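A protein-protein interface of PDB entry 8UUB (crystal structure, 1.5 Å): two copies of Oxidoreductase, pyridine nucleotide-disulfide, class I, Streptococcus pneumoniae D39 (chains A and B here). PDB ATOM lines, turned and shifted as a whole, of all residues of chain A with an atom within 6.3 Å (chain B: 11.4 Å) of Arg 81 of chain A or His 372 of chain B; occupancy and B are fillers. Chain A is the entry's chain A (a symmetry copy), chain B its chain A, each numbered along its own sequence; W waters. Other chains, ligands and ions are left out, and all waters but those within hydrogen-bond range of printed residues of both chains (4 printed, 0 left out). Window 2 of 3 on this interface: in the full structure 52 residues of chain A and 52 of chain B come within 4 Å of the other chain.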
ATOM      1  N   THR A  57      -6.937 -13.385 -28.590  1.00  0.00           N
ATOM      2  CA  THR A  57      -7.423 -14.258 -29.669  1.00  0.00           C
ATOM      3  C   THR A  57      -6.875 -13.782 -31.017  1.00  0.00           C
ATOM      4  O   THR A  57      -6.469 -14.580 -31.894  1.00  0.00           O
ATOM      5  CB  THR A  57      -8.964 -14.188 -29.732  1.00  0.00           C
ATOM      6  OG1 THR A  57      -9.454 -14.705 -28.497  1.00  0.00           O
ATOM      7  CG2 THR A  57      -9.536 -14.976 -30.915  1.00  0.00           C
ATOM      8  N   ASN A  76     -14.323 -12.376 -33.737  1.00  0.00           N
ATOM      9  CA  ASN A  76     -15.757 -12.174 -33.515  1.00  0.00           C
ATOM     10  C   ASN A  76     -16.480 -13.464 -33.115  1.00  0.00           C
ATOM     11  O   ASN A  76     -17.369 -13.456 -32.270  1.00  0.00           O
ATOM     12  CB  ASN A  76     -16.424 -11.552 -34.732  1.00  0.00           C
ATOM     13  CG  ASN A  76     -15.978 -10.120 -34.956  1.00  0.00           C
ATOM     14  OD1 ASN A  76     -15.569  -9.458 -33.984  1.00  0.00           O
ATOM     15  ND2 ASN A  76     -16.046  -9.658 -36.189  1.00  0.00           N
ATOM     16  N   THR A  77     -16.053 -14.591 -33.668  1.00  0.00           N
ATOM     17  CA  THR A  77     -16.683 -15.843 -33.248  1.00  0.00           C
ATOM     18  C   THR A  77     -16.415 -16.125 -31.769  1.00  0.00           C
ATOM     19  O   THR A  77     -17.343 -16.496 -31.015  1.00  0.00           O
ATOM     20  CB  THR A  77     -16.060 -16.988 -34.051  1.00  0.00           C
ATOM     21  OG1 THR A  77     -16.486 -16.806 -35.419  1.00  0.00           O
ATOM     22  CG2 THR A  77     -16.570 -18.354 -33.577  1.00  0.00           C
ATOM     23  N   ILE A  78     -15.158 -15.962 -31.336  1.00  0.00           N
ATOM     24  CA  ILE A  78     -14.768 -16.321 -29.971  1.00  0.00           C
ATOM     25  C   ILE A  78     -15.420 -15.371 -28.960  1.00  0.00           C
ATOM     26  O   ILE A  78     -15.951 -15.878 -27.972  1.00  0.00           O
ATOM     27  CB  ILE A  78     -13.228 -16.245 -29.897  1.00  0.00           C
ATOM     28  CG1 ILE A  78     -12.599 -17.318 -30.783  1.00  0.00           C
ATOM     29  CG2 ILE A  78     -12.753 -16.342 -28.439  1.00  0.00           C
ATOM     30  CD1 ILE A  78     -13.107 -18.713 -30.505  1.00  0.00           C
ATOM     31  N   THR A  79     -15.402 -14.063 -29.246  1.00  0.00           N
ATOM     32  CA  THR A  79     -16.003 -13.160 -28.273  1.00  0.00           C
ATOM     33  C   THR A  79     -17.515 -13.281 -28.271  1.00  0.00           C
ATOM     34  O   THR A  79     -18.146 -13.189 -27.209  1.00  0.00           O
ATOM     35  CB  THR A  79     -15.632 -11.690 -28.464  1.00  0.00           C
ATOM     36  OG1 THR A  79     -16.186 -11.174 -29.670  1.00  0.00           O
ATOM     37  CG2 THR A  79     -14.132 -11.436 -28.395  1.00  0.00           C
ATOM     38  N   GLY A  80     -18.096 -13.521 -29.451  1.00  0.00           N
ATOM     39  CA  GLY A  80     -19.543 -13.685 -29.520  1.00  0.00           C
ATOM     40  C   GLY A  80     -20.003 -14.894 -28.727  1.00  0.00           C
ATOM     41  O   GLY A  80     -21.044 -14.872 -28.022  1.00  0.00           O
ATOM     42  N   ARG A  81     -19.242 -16.008 -28.812  1.00  0.00           N
ATOM     43  CA  ARG A  81     -19.646 -17.179 -28.043  1.00  0.00           C
ATOM     44  C   ARG A  81     -19.533 -16.931 -26.540  1.00  0.00           C
ATOM     45  O   ARG A  81     -20.458 -17.277 -25.791  1.00  0.00           O
ATOM     46  CB  ARG A  81     -18.789 -18.376 -28.474  1.00  0.00           C
ATOM     47  CG  ARG A  81     -19.227 -19.647 -27.771  1.00  0.00           C
ATOM     48  CD  ARG A  81     -18.336 -20.856 -28.080  1.00  0.00           C
ATOM     49  NE  ARG A  81     -18.341 -21.189 -29.481  1.00  0.00           N
ATOM     50  CZ  ARG A  81     -17.329 -21.048 -30.323  1.00  0.00           C
ATOM     51  NH1 ARG A  81     -16.184 -20.443 -29.953  1.00  0.00           N
ATOM     52  NH2 ARG A  81     -17.451 -21.565 -31.556  1.00  0.00           N
ATOM     53  N   LEU A  82     -18.421 -16.304 -26.118  1.00  0.00           N
ATOM     54  CA  LEU A  82     -18.288 -16.016 -24.695  1.00  0.00           C
ATOM     55  C   LEU A  82     -19.290 -14.969 -24.213  1.00  0.00           C
ATOM     56  O   LEU A  82     -19.739 -15.050 -23.057  1.00  0.00           O
ATOM     57  CB  LEU A  82     -16.843 -15.584 -24.400  1.00  0.00           C
ATOM     58  CG  LEU A  82     -15.888 -16.794 -24.336  1.00  0.00           C
ATOM     59  CD1 LEU A  82     -14.454 -16.306 -24.507  1.00  0.00           C
ATOM     60  CD2 LEU A  82     -16.017 -17.509 -22.974  1.00  0.00           C
ATOM     61  N   ASN A  83     -19.693 -14.047 -25.089  1.00  0.00           N
ATOM     62  CA  ASN A  83     -20.746 -13.068 -24.732  1.00  0.00           C
ATOM     63  C   ASN A  83     -22.046 -13.803 -24.425  1.00  0.00           C
ATOM     64  O   ASN A  83     -22.669 -13.618 -23.360  1.00  0.00           O
ATOM     65  CB  ASN A  83     -20.835 -12.095 -25.907  1.00  0.00           C
ATOM     66  CG  ASN A  83     -21.969 -11.082 -25.845  1.00  0.00           C
ATOM     67  OD1 ASN A  83     -23.149 -11.499 -25.817  1.00  0.00           O
ATOM     68  ND2 ASN A  83     -21.656  -9.778 -25.895  1.00  0.00           N
ATOM     69  N   GLY A  84     -22.430 -14.748 -25.289  1.00  0.00           N
ATOM     70  CA  GLY A  84     -23.664 -15.482 -25.053  1.00  0.00           C
ATOM     71  C   GLY A  84     -23.540 -16.438 -23.871  1.00  0.00           C
ATOM     72  O   GLY A  84     -24.485 -16.650 -23.114  1.00  0.00           O
ATOM     73  N   LYS A  85     -22.365 -17.053 -23.687  1.00  0.00           N
ATOM     74  CA  LYS A  85     -22.130 -17.949 -22.579  1.00  0.00           C
ATOM     75  C   LYS A  85     -22.282 -17.160 -21.263  1.00  0.00           C
ATOM     76  O   LYS A  85     -22.908 -17.647 -20.317  1.00  0.00           O
ATOM     77  CB  LYS A  85     -20.712 -18.548 -22.613  1.00  0.00           C
ATOM     78  CG  LYS A  85     -20.528 -19.546 -21.496  1.00  0.00           C
ATOM     79  CD  LYS A  85     -19.118 -20.206 -21.437  1.00  0.00           C
ATOM     80  CE  LYS A  85     -18.930 -21.101 -20.218  1.00  0.00           C
ATOM     81  NZ  LYS A  85     -17.648 -21.885 -20.264  1.00  0.00           N
ATOM     82  N   ASN A  86     -21.771 -15.913 -21.253  1.00  0.00           N
ATOM     83  CA  ASN A  86     -21.896 -15.136 -20.005  1.00  0.00           C
ATOM     84  C   ASN A  86     -23.314 -14.672 -19.725  1.00  0.00           C
ATOM     85  O   ASN A  86     -23.794 -14.835 -18.605  1.00  0.00           O
ATOM     86  CB  ASN A  86     -20.996 -13.884 -20.068  1.00  0.00           C
ATOM     87  CG  ASN A  86     -19.630 -14.275 -19.579  1.00  0.00           C
ATOM     88  OD1 ASN A  86     -19.330 -14.083 -18.397  1.00  0.00           O
ATOM     89  ND2 ASN A  86     -18.780 -14.853 -20.415  1.00  0.00           N
ATOM     90  N   ILE B 363     -12.310 -30.232 -14.979  1.00  0.00           N
ATOM     91  CA  ILE B 363     -12.806 -29.169 -15.856  1.00  0.00           C
ATOM     92  C   ILE B 363     -12.189 -29.422 -17.227  1.00  0.00           C
ATOM     93  O   ILE B 363     -10.952 -29.476 -17.325  1.00  0.00           O
ATOM     94  CB  ILE B 363     -12.394 -27.769 -15.372  1.00  0.00           C
ATOM     95  CG1 ILE B 363     -12.936 -27.546 -13.944  1.00  0.00           C
ATOM     96  CG2 ILE B 363     -12.890 -26.720 -16.375  1.00  0.00           C
ATOM     97  CD1 ILE B 363     -12.465 -26.206 -13.301  1.00  0.00           C
ATOM     98  N   PRO B 364     -12.948 -29.570 -18.324  1.00  0.00           N
ATOM     99  CA  PRO B 364     -12.379 -29.707 -19.666  1.00  0.00           C
ATOM    100  C   PRO B 364     -11.823 -28.373 -20.151  1.00  0.00           C
ATOM    101  O   PRO B 364     -12.333 -27.287 -19.829  1.00  0.00           O
ATOM    102  CB  PRO B 364     -13.559 -30.116 -20.562  1.00  0.00           C
ATOM    103  CG  PRO B 364     -14.743 -29.557 -19.791  1.00  0.00           C
ATOM    104  CD  PRO B 364     -14.436 -29.548 -18.310  1.00  0.00           C
ATOM    105  N   VAL B 365     -10.753 -28.425 -20.958  1.00  0.00           N
ATOM    106  CA  VAL B 365     -10.188 -27.214 -21.561  1.00  0.00           C
ATOM    107  C   VAL B 365     -11.250 -26.557 -22.443  1.00  0.00           C
ATOM    108  O   VAL B 365     -11.247 -25.323 -22.594  1.00  0.00           O
ATOM    109  CB  VAL B 365      -8.935 -27.589 -22.377  1.00  0.00           C
ATOM    110  CG1 VAL B 365      -8.466 -26.465 -23.322  1.00  0.00           C
ATOM    111  CG2 VAL B 365      -7.823 -27.887 -21.375  1.00  0.00           C
ATOM    112  N   ALA B 366     -12.210 -27.369 -22.935  1.00  0.00           N
ATOM    113  CA  ALA B 366     -13.253 -26.784 -23.770  1.00  0.00           C
ATOM    114  C   ALA B 366     -14.117 -25.776 -22.995  1.00  0.00           C
ATOM    115  O   ALA B 366     -14.853 -25.005 -23.654  1.00  0.00           O
ATOM    116  CB  ALA B 366     -14.115 -27.900 -24.371  1.00  0.00           C
ATOM    117  N   ALA B 367     -14.134 -25.816 -21.658  1.00  0.00           N
ATOM    118  CA  ALA B 367     -14.907 -24.915 -20.841  1.00  0.00           C
ATOM    119  C   ALA B 367     -14.053 -23.742 -20.389  1.00  0.00           C
ATOM    120  O   ALA B 367     -14.542 -22.887 -19.622  1.00  0.00           O
ATOM    121  CB  ALA B 367     -15.454 -25.598 -19.587  1.00  0.00           C
ATOM    122  N   MET B 368     -12.818 -23.621 -20.894  1.00  0.00           N
ATOM    123  CA  MET B 368     -11.919 -22.594 -20.357  1.00  0.00           C
ATOM    124  C   MET B 368     -11.711 -21.489 -21.399  1.00  0.00           C
ATOM    125  O   MET B 368     -11.405 -21.800 -22.566  1.00  0.00           O
ATOM    126  CB  MET B 368     -10.512 -23.172 -20.055  1.00  0.00           C
ATOM    127  CG  MET B 368     -10.607 -24.227 -18.982  1.00  0.00           C
ATOM    128  SD  MET B 368      -8.974 -24.970 -18.682  1.00  0.00           S
ATOM    129  CE  MET B 368      -9.399 -26.357 -17.616  1.00  0.00           C
ATOM    130  N   PRO B 369     -11.902 -20.167 -21.062  1.00  0.00           N
ATOM    131  CA  PRO B 369     -11.773 -19.131 -22.072  1.00  0.00           C
ATOM    132  C   PRO B 369     -10.461 -19.176 -22.850  1.00  0.00           C
ATOM    133  O   PRO B 369     -10.467 -18.970 -24.069  1.00  0.00           O
ATOM    134  CB  PRO B 369     -11.946 -17.809 -21.280  1.00  0.00           C
ATOM    135  CG  PRO B 369     -12.876 -18.251 -20.133  1.00  0.00           C
ATOM    136  CD  PRO B 369     -12.442 -19.687 -19.772  1.00  0.00           C
ATOM    137  N   ARG B 370      -9.339 -19.485 -22.142  1.00  0.00           N
ATOM    138  CA  ARG B 370      -8.067 -19.502 -22.868  1.00  0.00           C
ATOM    139  C   ARG B 370      -8.055 -20.620 -23.920  1.00  0.00           C
ATOM    140  O   ARG B 370      -7.329 -20.471 -24.916  1.00  0.00           O
ATOM    141  CB  ARG B 370      -6.874 -19.604 -21.892  1.00  0.00           C
ATOM    142  CG  ARG B 370      -5.520 -19.602 -22.629  1.00  0.00           C
ATOM    143  CD  ARG B 370      -5.132 -18.222 -23.150  1.00  0.00           C
ATOM    144  NE  ARG B 370      -4.072 -18.338 -24.143  1.00  0.00           N
ATOM    145  CZ  ARG B 370      -3.264 -17.391 -24.430  1.00  0.00           C
ATOM    146  NH1 ARG B 370      -3.168 -16.281 -23.658  1.00  0.00           N
ATOM    147  NH2 ARG B 370      -2.524 -17.546 -25.529  1.00  0.00           N
ATOM    148  N   GLY B 371      -8.759 -21.739 -23.695  1.00  0.00           N
ATOM    149  CA  GLY B 371      -8.810 -22.734 -24.774  1.00  0.00           C
ATOM    150  C   GLY B 371      -9.426 -22.151 -26.062  1.00  0.00           C
ATOM    151  O   GLY B 371      -8.895 -22.358 -27.165  1.00  0.00           O
ATOM    152  N   HIS B 372     -10.477 -21.339 -25.909  1.00  0.00           N
ATOM    153  CA  HIS B 372     -11.064 -20.708 -27.076  1.00  0.00           C
ATOM    154  C   HIS B 372     -10.119 -19.678 -27.711  1.00  0.00           C
ATOM    155  O   HIS B 372      -9.985 -19.611 -28.923  1.00  0.00           O
ATOM    156  CB  HIS B 372     -12.407 -20.059 -26.670  1.00  0.00           C
ATOM    157  CG  HIS B 372     -13.363 -21.135 -26.275  1.00  0.00           C
ATOM    158  ND1 HIS B 372     -14.139 -21.804 -27.236  1.00  0.00           N
ATOM    159  CD2 HIS B 372     -13.563 -21.748 -25.079  1.00  0.00           C
ATOM    160  CE1 HIS B 372     -14.853 -22.750 -26.606  1.00  0.00           C
ATOM    161  NE2 HIS B 372     -14.547 -22.688 -25.261  1.00  0.00           N
ATOM    162  N   VAL B 373      -9.444 -18.873 -26.856  1.00  0.00           N
ATOM    163  CA  VAL B 373      -8.438 -17.932 -27.340  1.00  0.00           C
ATOM    164  C   VAL B 373      -7.394 -18.684 -28.185  1.00  0.00           C
ATOM    165  O   VAL B 373      -6.929 -18.160 -29.207  1.00  0.00           O
ATOM    166  CB  VAL B 373      -7.768 -17.288 -26.107  1.00  0.00           C
ATOM    167  CG1 VAL B 373      -6.510 -16.514 -26.505  1.00  0.00           C
ATOM    168  CG2 VAL B 373      -8.703 -16.338 -25.357  1.00  0.00           C
ATOM    169  N   ASN B 374      -6.974 -19.876 -27.692  1.00  0.00           N
ATOM    170  CA  ASN B 374      -5.915 -20.625 -28.355  1.00  0.00           C
ATOM    171  C   ASN B 374      -6.383 -21.298 -29.645  1.00  0.00           C
ATOM    172  O   ASN B 374      -5.540 -21.755 -30.424  1.00  0.00           O
ATOM    173  CB  ASN B 374      -5.463 -21.741 -27.416  1.00  0.00           C
ATOM    174  CG  ASN B 374      -4.566 -21.238 -26.291  1.00  0.00           C
ATOM    175  OD1 ASN B 374      -4.089 -20.093 -26.364  1.00  0.00           O
ATOM    176  ND2 ASN B 374      -4.337 -22.115 -25.339  1.00  0.00           N
ATOM    177  N   GLY B 375      -7.697 -21.354 -29.853  1.00  0.00           N
ATOM    178  CA  GLY B 375      -8.191 -22.140 -30.980  1.00  0.00           C
ATOM    179  C   GLY B 375      -7.951 -23.636 -30.761  1.00  0.00           C
ATOM    180  O   GLY B 375      -7.710 -24.360 -31.743  1.00  0.00           O
ATOM    181  N   ASP B 376      -7.844 -24.050 -29.505  1.00  0.00           N
ATOM    182  CA  ASP B 376      -7.494 -25.436 -29.197  1.00  0.00           C
ATOM    183  C   ASP B 376      -8.276 -25.815 -27.968  1.00  0.00           C
ATOM    184  O   ASP B 376      -7.954 -25.412 -26.845  1.00  0.00           O
ATOM    185  CB  ASP B 376      -5.983 -25.534 -28.910  1.00  0.00           C
ATOM    186  CG  ASP B 376      -5.584 -26.891 -28.355  1.00  0.00           C
ATOM    187  OD1 ASP B 376      -6.367 -27.862 -28.497  1.00  0.00           O
ATOM    188  OD2 ASP B 376      -4.449 -26.985 -27.801  1.00  0.00           O
ATOM    189  N   LEU B 377      -9.321 -26.656 -28.144  1.00  0.00           N
ATOM    190  CA  LEU B 377     -10.173 -27.010 -27.024  1.00  0.00           C
ATOM    191  C   LEU B 377      -9.781 -28.383 -26.480  1.00  0.00           C
ATOM    192  O   LEU B 377     -10.571 -28.958 -25.713  1.00  0.00           O
ATOM    193  CB  LEU B 377     -11.605 -27.078 -27.555  1.00  0.00           C
ATOM    194  CG  LEU B 377     -12.109 -25.734 -28.113  1.00  0.00           C
ATOM    195  CD1 LEU B 377     -13.611 -25.880 -28.386  1.00  0.00           C
ATOM    196  CD2 LEU B 377     -11.869 -24.572 -27.173  1.00  0.00           C
ATOM    197  N   ARG B 378      -8.595 -28.920 -26.812  1.00  0.00           N
ATOM    198  CA  ARG B 378      -8.191 -30.238 -26.311  1.00  0.00           C
ATOM    199  C   ARG B 378      -7.724 -30.173 -24.848  1.00  0.00           C
ATOM    200  O   ARG B 378      -6.886 -29.352 -24.442  1.00  0.00           O
ATOM    201  CB  ARG B 378      -7.030 -30.755 -27.154  1.00  0.00           C
ATOM    202  CG  ARG B 378      -7.528 -31.284 -28.504  1.00  0.00           C
ATOM    203  CD  ARG B 378      -6.346 -31.852 -29.270  1.00  0.00           C
ATOM    204  NE  ARG B 378      -6.910 -32.530 -30.460  1.00  0.00           N
ATOM    205  CZ  ARG B 378      -6.152 -33.265 -31.307  1.00  0.00           C
ATOM    206  NH1 ARG B 378      -4.834 -33.434 -31.147  1.00  0.00           N
ATOM    207  NH2 ARG B 378      -6.730 -33.842 -32.343  1.00  0.00           N
ATOM    208  N   GLY B 379      -8.218 -31.154 -24.098  1.00  0.00           N
ATOM    209  CA  GLY B 379      -7.606 -31.476 -22.816  1.00  0.00           C
ATOM    210  C   GLY B 379      -8.555 -31.317 -21.627  1.00  0.00           C
ATOM    211  O   GLY B 379      -9.768 -31.067 -21.766  1.00  0.00           O
ATOM    212  N   PHE B 381      -8.307 -30.603 -16.926  1.00  0.00           N
ATOM    213  CA  PHE B 381      -7.642 -30.569 -15.646  1.00  0.00           C
ATOM    214  C   PHE B 381      -8.410 -31.462 -14.686  1.00  0.00           C
ATOM    215  O   PHE B 381      -9.650 -31.402 -14.697  1.00  0.00           O
ATOM    216  CB  PHE B 381      -7.598 -29.170 -15.047  1.00  0.00           C
ATOM    217  CG  PHE B 381      -6.802 -28.060 -15.735  1.00  0.00           C
ATOM    218  CD1 PHE B 381      -6.134 -28.237 -16.922  1.00  0.00           C
ATOM    219  CD2 PHE B 381      -6.736 -26.813 -15.101  1.00  0.00           C
ATOM    220  CE1 PHE B 381      -5.405 -27.175 -17.491  1.00  0.00           C
ATOM    221  CE2 PHE B 381      -6.025 -25.764 -15.649  1.00  0.00           C
ATOM    222  CZ  PHE B 381      -5.383 -25.955 -16.863  1.00  0.00           C
ATOM    223  N   SER B 399      -3.112 -30.257 -21.483  1.00  0.00           N
ATOM    224  CA  SER B 399      -3.422 -28.991 -22.135  1.00  0.00           C
ATOM    225  C   SER B 399      -2.158 -28.411 -22.760  1.00  0.00           C
ATOM    226  O   SER B 399      -1.039 -28.762 -22.328  1.00  0.00           O
ATOM    227  CB  SER B 399      -4.029 -27.943 -21.168  1.00  0.00           C
ATOM    228  OG  SER B 399      -3.022 -27.361 -20.300  1.00  0.00           O
ATOM    229  N   GLU B 400      -2.357 -27.430 -23.638  1.00  0.00           N
ATOM    230  CA  GLU B 400      -1.264 -26.568 -24.075  1.00  0.00           C
ATOM    231  C   GLU B 400      -0.555 -26.020 -22.822  1.00  0.00           C
ATOM    232  O   GLU B 400      -1.194 -25.548 -21.879  1.00  0.00           O
ATOM    233  CB  GLU B 400      -1.892 -25.426 -24.888  1.00  0.00           C
ATOM    234  CG  GLU B 400      -0.865 -24.361 -25.325  1.00  0.00           C
ATOM    235  CD  GLU B 400       0.119 -24.939 -26.326  1.00  0.00           C
ATOM    236  OE1 GLU B 400      -0.316 -25.502 -27.378  1.00  0.00           O
ATOM    237  OE2 GLU B 400       1.333 -24.725 -26.120  1.00  0.00           O
ATOM    238  N   HIS B 429      -4.251 -13.524 -16.577  1.00  0.00           N
ATOM    239  CA  HIS B 429      -5.421 -13.787 -17.404  1.00  0.00           C
ATOM    240  C   HIS B 429      -5.203 -13.083 -18.731  1.00  0.00           C
ATOM    241  O   HIS B 429      -4.681 -11.953 -18.736  1.00  0.00           O
ATOM    242  CB  HIS B 429      -6.623 -13.140 -16.697  1.00  0.00           C
ATOM    243  CG  HIS B 429      -7.912 -13.114 -17.434  1.00  0.00           C
ATOM    244  ND1 HIS B 429      -8.929 -13.974 -17.100  1.00  0.00           N
ATOM    245  CD2 HIS B 429      -8.420 -12.231 -18.324  1.00  0.00           C
ATOM    246  CE1 HIS B 429      -9.987 -13.713 -17.854  1.00  0.00           C
ATOM    247  NE2 HIS B 429      -9.709 -12.635 -18.587  1.00  0.00           N
ATOM    248  N   PRO B 430      -5.557 -13.674 -19.897  1.00  0.00           N
ATOM    249  CA  PRO B 430      -6.161 -15.000 -19.983  1.00  0.00           C
ATOM    250  C   PRO B 430      -5.076 -16.054 -20.091  1.00  0.00           C
ATOM    251  O   PRO B 430      -4.181 -15.940 -20.928  1.00  0.00           O
ATOM    252  CB  PRO B 430      -6.976 -14.894 -21.318  1.00  0.00           C
ATOM    253  CG  PRO B 430      -6.213 -13.878 -22.112  1.00  0.00           C
ATOM    254  CD  PRO B 430      -5.377 -12.991 -21.178  1.00  0.00           C
ATOM    255  N   THR B 431      -5.209 -17.080 -19.276  1.00  0.00           N
ATOM    256  CA  THR B 431      -4.220 -18.178 -19.221  1.00  0.00           C
ATOM    257  C   THR B 431      -4.969 -19.478 -18.967  1.00  0.00           C
ATOM    258  O   THR B 431      -6.164 -19.491 -18.659  1.00  0.00           O
ATOM    259  CB  THR B 431      -3.183 -17.993 -18.084  1.00  0.00           C
ATOM    260  OG1 THR B 431      -3.899 -18.032 -16.825  1.00  0.00           O
ATOM    261  CG2 THR B 431      -2.458 -16.675 -18.210  1.00  0.00           C
ATOM    262  N   LEU B 432      -4.284 -20.618 -19.164  1.00  0.00           N
ATOM    263  CA  LEU B 432      -4.888 -21.861 -18.676  1.00  0.00           C
ATOM    264  C   LEU B 432      -4.719 -22.027 -17.170  1.00  0.00           C
ATOM    265  O   LEU B 432      -5.630 -22.556 -16.506  1.00  0.00           O
ATOM    266  CB  LEU B 432      -4.363 -23.044 -19.504  1.00  0.00           C
ATOM    267  CG  LEU B 432      -4.956 -23.045 -20.914  1.00  0.00           C
ATOM    268  CD1 LEU B 432      -4.244 -24.029 -21.813  1.00  0.00           C
ATOM    269  CD2 LEU B 432      -6.423 -23.395 -20.892  1.00  0.00           C
ATOM    270  N   GLU B 434      -5.125 -19.957 -14.751  1.00  0.00           N
ATOM    271  CA  GLU B 434      -6.081 -19.344 -13.839  1.00  0.00           C
ATOM    272  C   GLU B 434      -7.249 -20.289 -13.555  1.00  0.00           C
ATOM    273  O   GLU B 434      -7.972 -20.149 -12.562  1.00  0.00           O
ATOM    274  CB  GLU B 434      -6.595 -18.039 -14.427  1.00  0.00           C
ATOM    275  CG  GLU B 434      -7.333 -18.259 -15.741  1.00  0.00           C
ATOM    276  CD  GLU B 434      -7.683 -16.923 -16.338  1.00  0.00           C
ATOM    277  OE1 GLU B 434      -8.155 -16.065 -15.555  1.00  0.00           O
ATOM    278  OE2 GLU B 434      -7.506 -16.752 -17.580  1.00  0.00           O
ATOM    279  N   ASN B 435      -7.463 -21.254 -14.440  1.00  0.00           N
ATOM    280  CA  ASN B 435      -8.578 -22.161 -14.163  1.00  0.00           C
ATOM    281  C   ASN B 435      -8.357 -23.005 -12.912  1.00  0.00           C
ATOM    282  O   ASN B 435      -9.317 -23.633 -12.457  1.00  0.00           O
ATOM    283  CB  ASN B 435      -8.940 -23.008 -15.389  1.00  0.00           C
ATOM    284  CG  ASN B 435      -9.349 -22.136 -16.546  1.00  0.00           C
ATOM    285  OD1 ASN B 435     -10.525 -21.747 -16.609  1.00  0.00           O
ATOM    286  ND2 ASN B 435      -8.414 -21.693 -17.364  1.00  0.00           N
HETATM  287  O   HOH W   1      -7.238 -17.380 -31.865  1.00  0.00           O
HETATM  288  O   HOH W   2     -15.535 -18.831 -27.538  1.00  0.00           O
HETATM  289  O   HOH W   3     -17.043 -22.887 -22.858  1.00  0.00           O
HETATM  290  O   HOH W   4     -15.174 -20.860 -22.327  1.00  0.00           O
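No residue of chain B comes within 4 Å of Thr 77 of chain A.
Printed residues of chain B within 4 Å of Ile 78 of chain A: His 372 (3.6 Å).
No residue of chain B comes within 4 Å of Thr 79 of chain A.
No residue of chain B comes within 4 Å of Gly 80 of chain A.
No residue of chain B comes within 4 Å of Leu 82 of chain A.
No residue of chain B comes within 4 Å of Asn 83 of chain A.
Of chain B, only Ala 367 (3.3 Å) comes within 4 Å of Lys 85 of chain A.
Of the printed residues of chain A, Ala 367 of chain B touches Lys 85 (3.3 Å).
Of the printed residues of chain A, His 372 of chain B touches Ile 78 and Arg 81.
Asn 435 of chain B touches none of the printed residues of chain A.
The nearest residue of chain B that does not touch Arg 81 of chain A is Leu 377 of chain B (6.2 Å).
The side-chain amino group (NZ) of Lys 85 of chain A is in hydrogen-bond range of the backbone carbonyl oxygen (O) of Ala 367 of chain B.
Printed residues of chain B that touch a printed residue of chain A: Ala 367, His 372 and Val 373.
Hydrophobic or aromatic side chains of chain B within 4 Å of the printed part of chain A: His 372 and Val 373.
Hydrophobic or aromatic side chains of chain A that line the printed part of chain B: Ile 78.
Among the printed residues, 4 pairs touch across the chains.
Among the printed residues, no Asp or Glu carboxylate lies within 4 Å of a Lys or Arg side-chain nitrogen of the other chain.
Water W1 bridges the backbone carbonyl oxygen of Val 373 of chain B (2.8 Å) and the backbone carbonyl oxygen of Thr 57 of chain A (2.9 Å).
Water W3 lies within hydrogen-bond range of the side-chain amino group (NZ) of Lys 85 of chain A (2.8 Å), the backbone carbonyl oxygen (O) of Ala 366 of chain B (3.1 Å) and a ring nitrogen (NE2) of His 372 of chain B (3.5 Å).
Water W2 lies within hydrogen-bond range of the guanidinium group of Arg 81 of chain A (3.0 Å), the backbone carbonyl oxygen of Ile 78 of chain A (3.0 Å) and a ring nitrogen (ND1) of His 372 of chain B (3.3 Å).
Water W4 lies within hydrogen-bond range of NZ of Lys 85 of chain A (3.4 Å) and O of Ala 367 of chain B (3.4 Å).
Val 373 of chain B touches Thr 57 of chain A.
Ile 78 of chain A touches His 372 of chain B.
Arg 81 of chain A touches His 372 of chain B (NH1 to ND1, 3.7 Å).
No position is printed for both chains.
O of Ala 366 of chain B sits at hydrogen-bond distance from NE2 of His 372 of chain B, 2.8 Å away.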
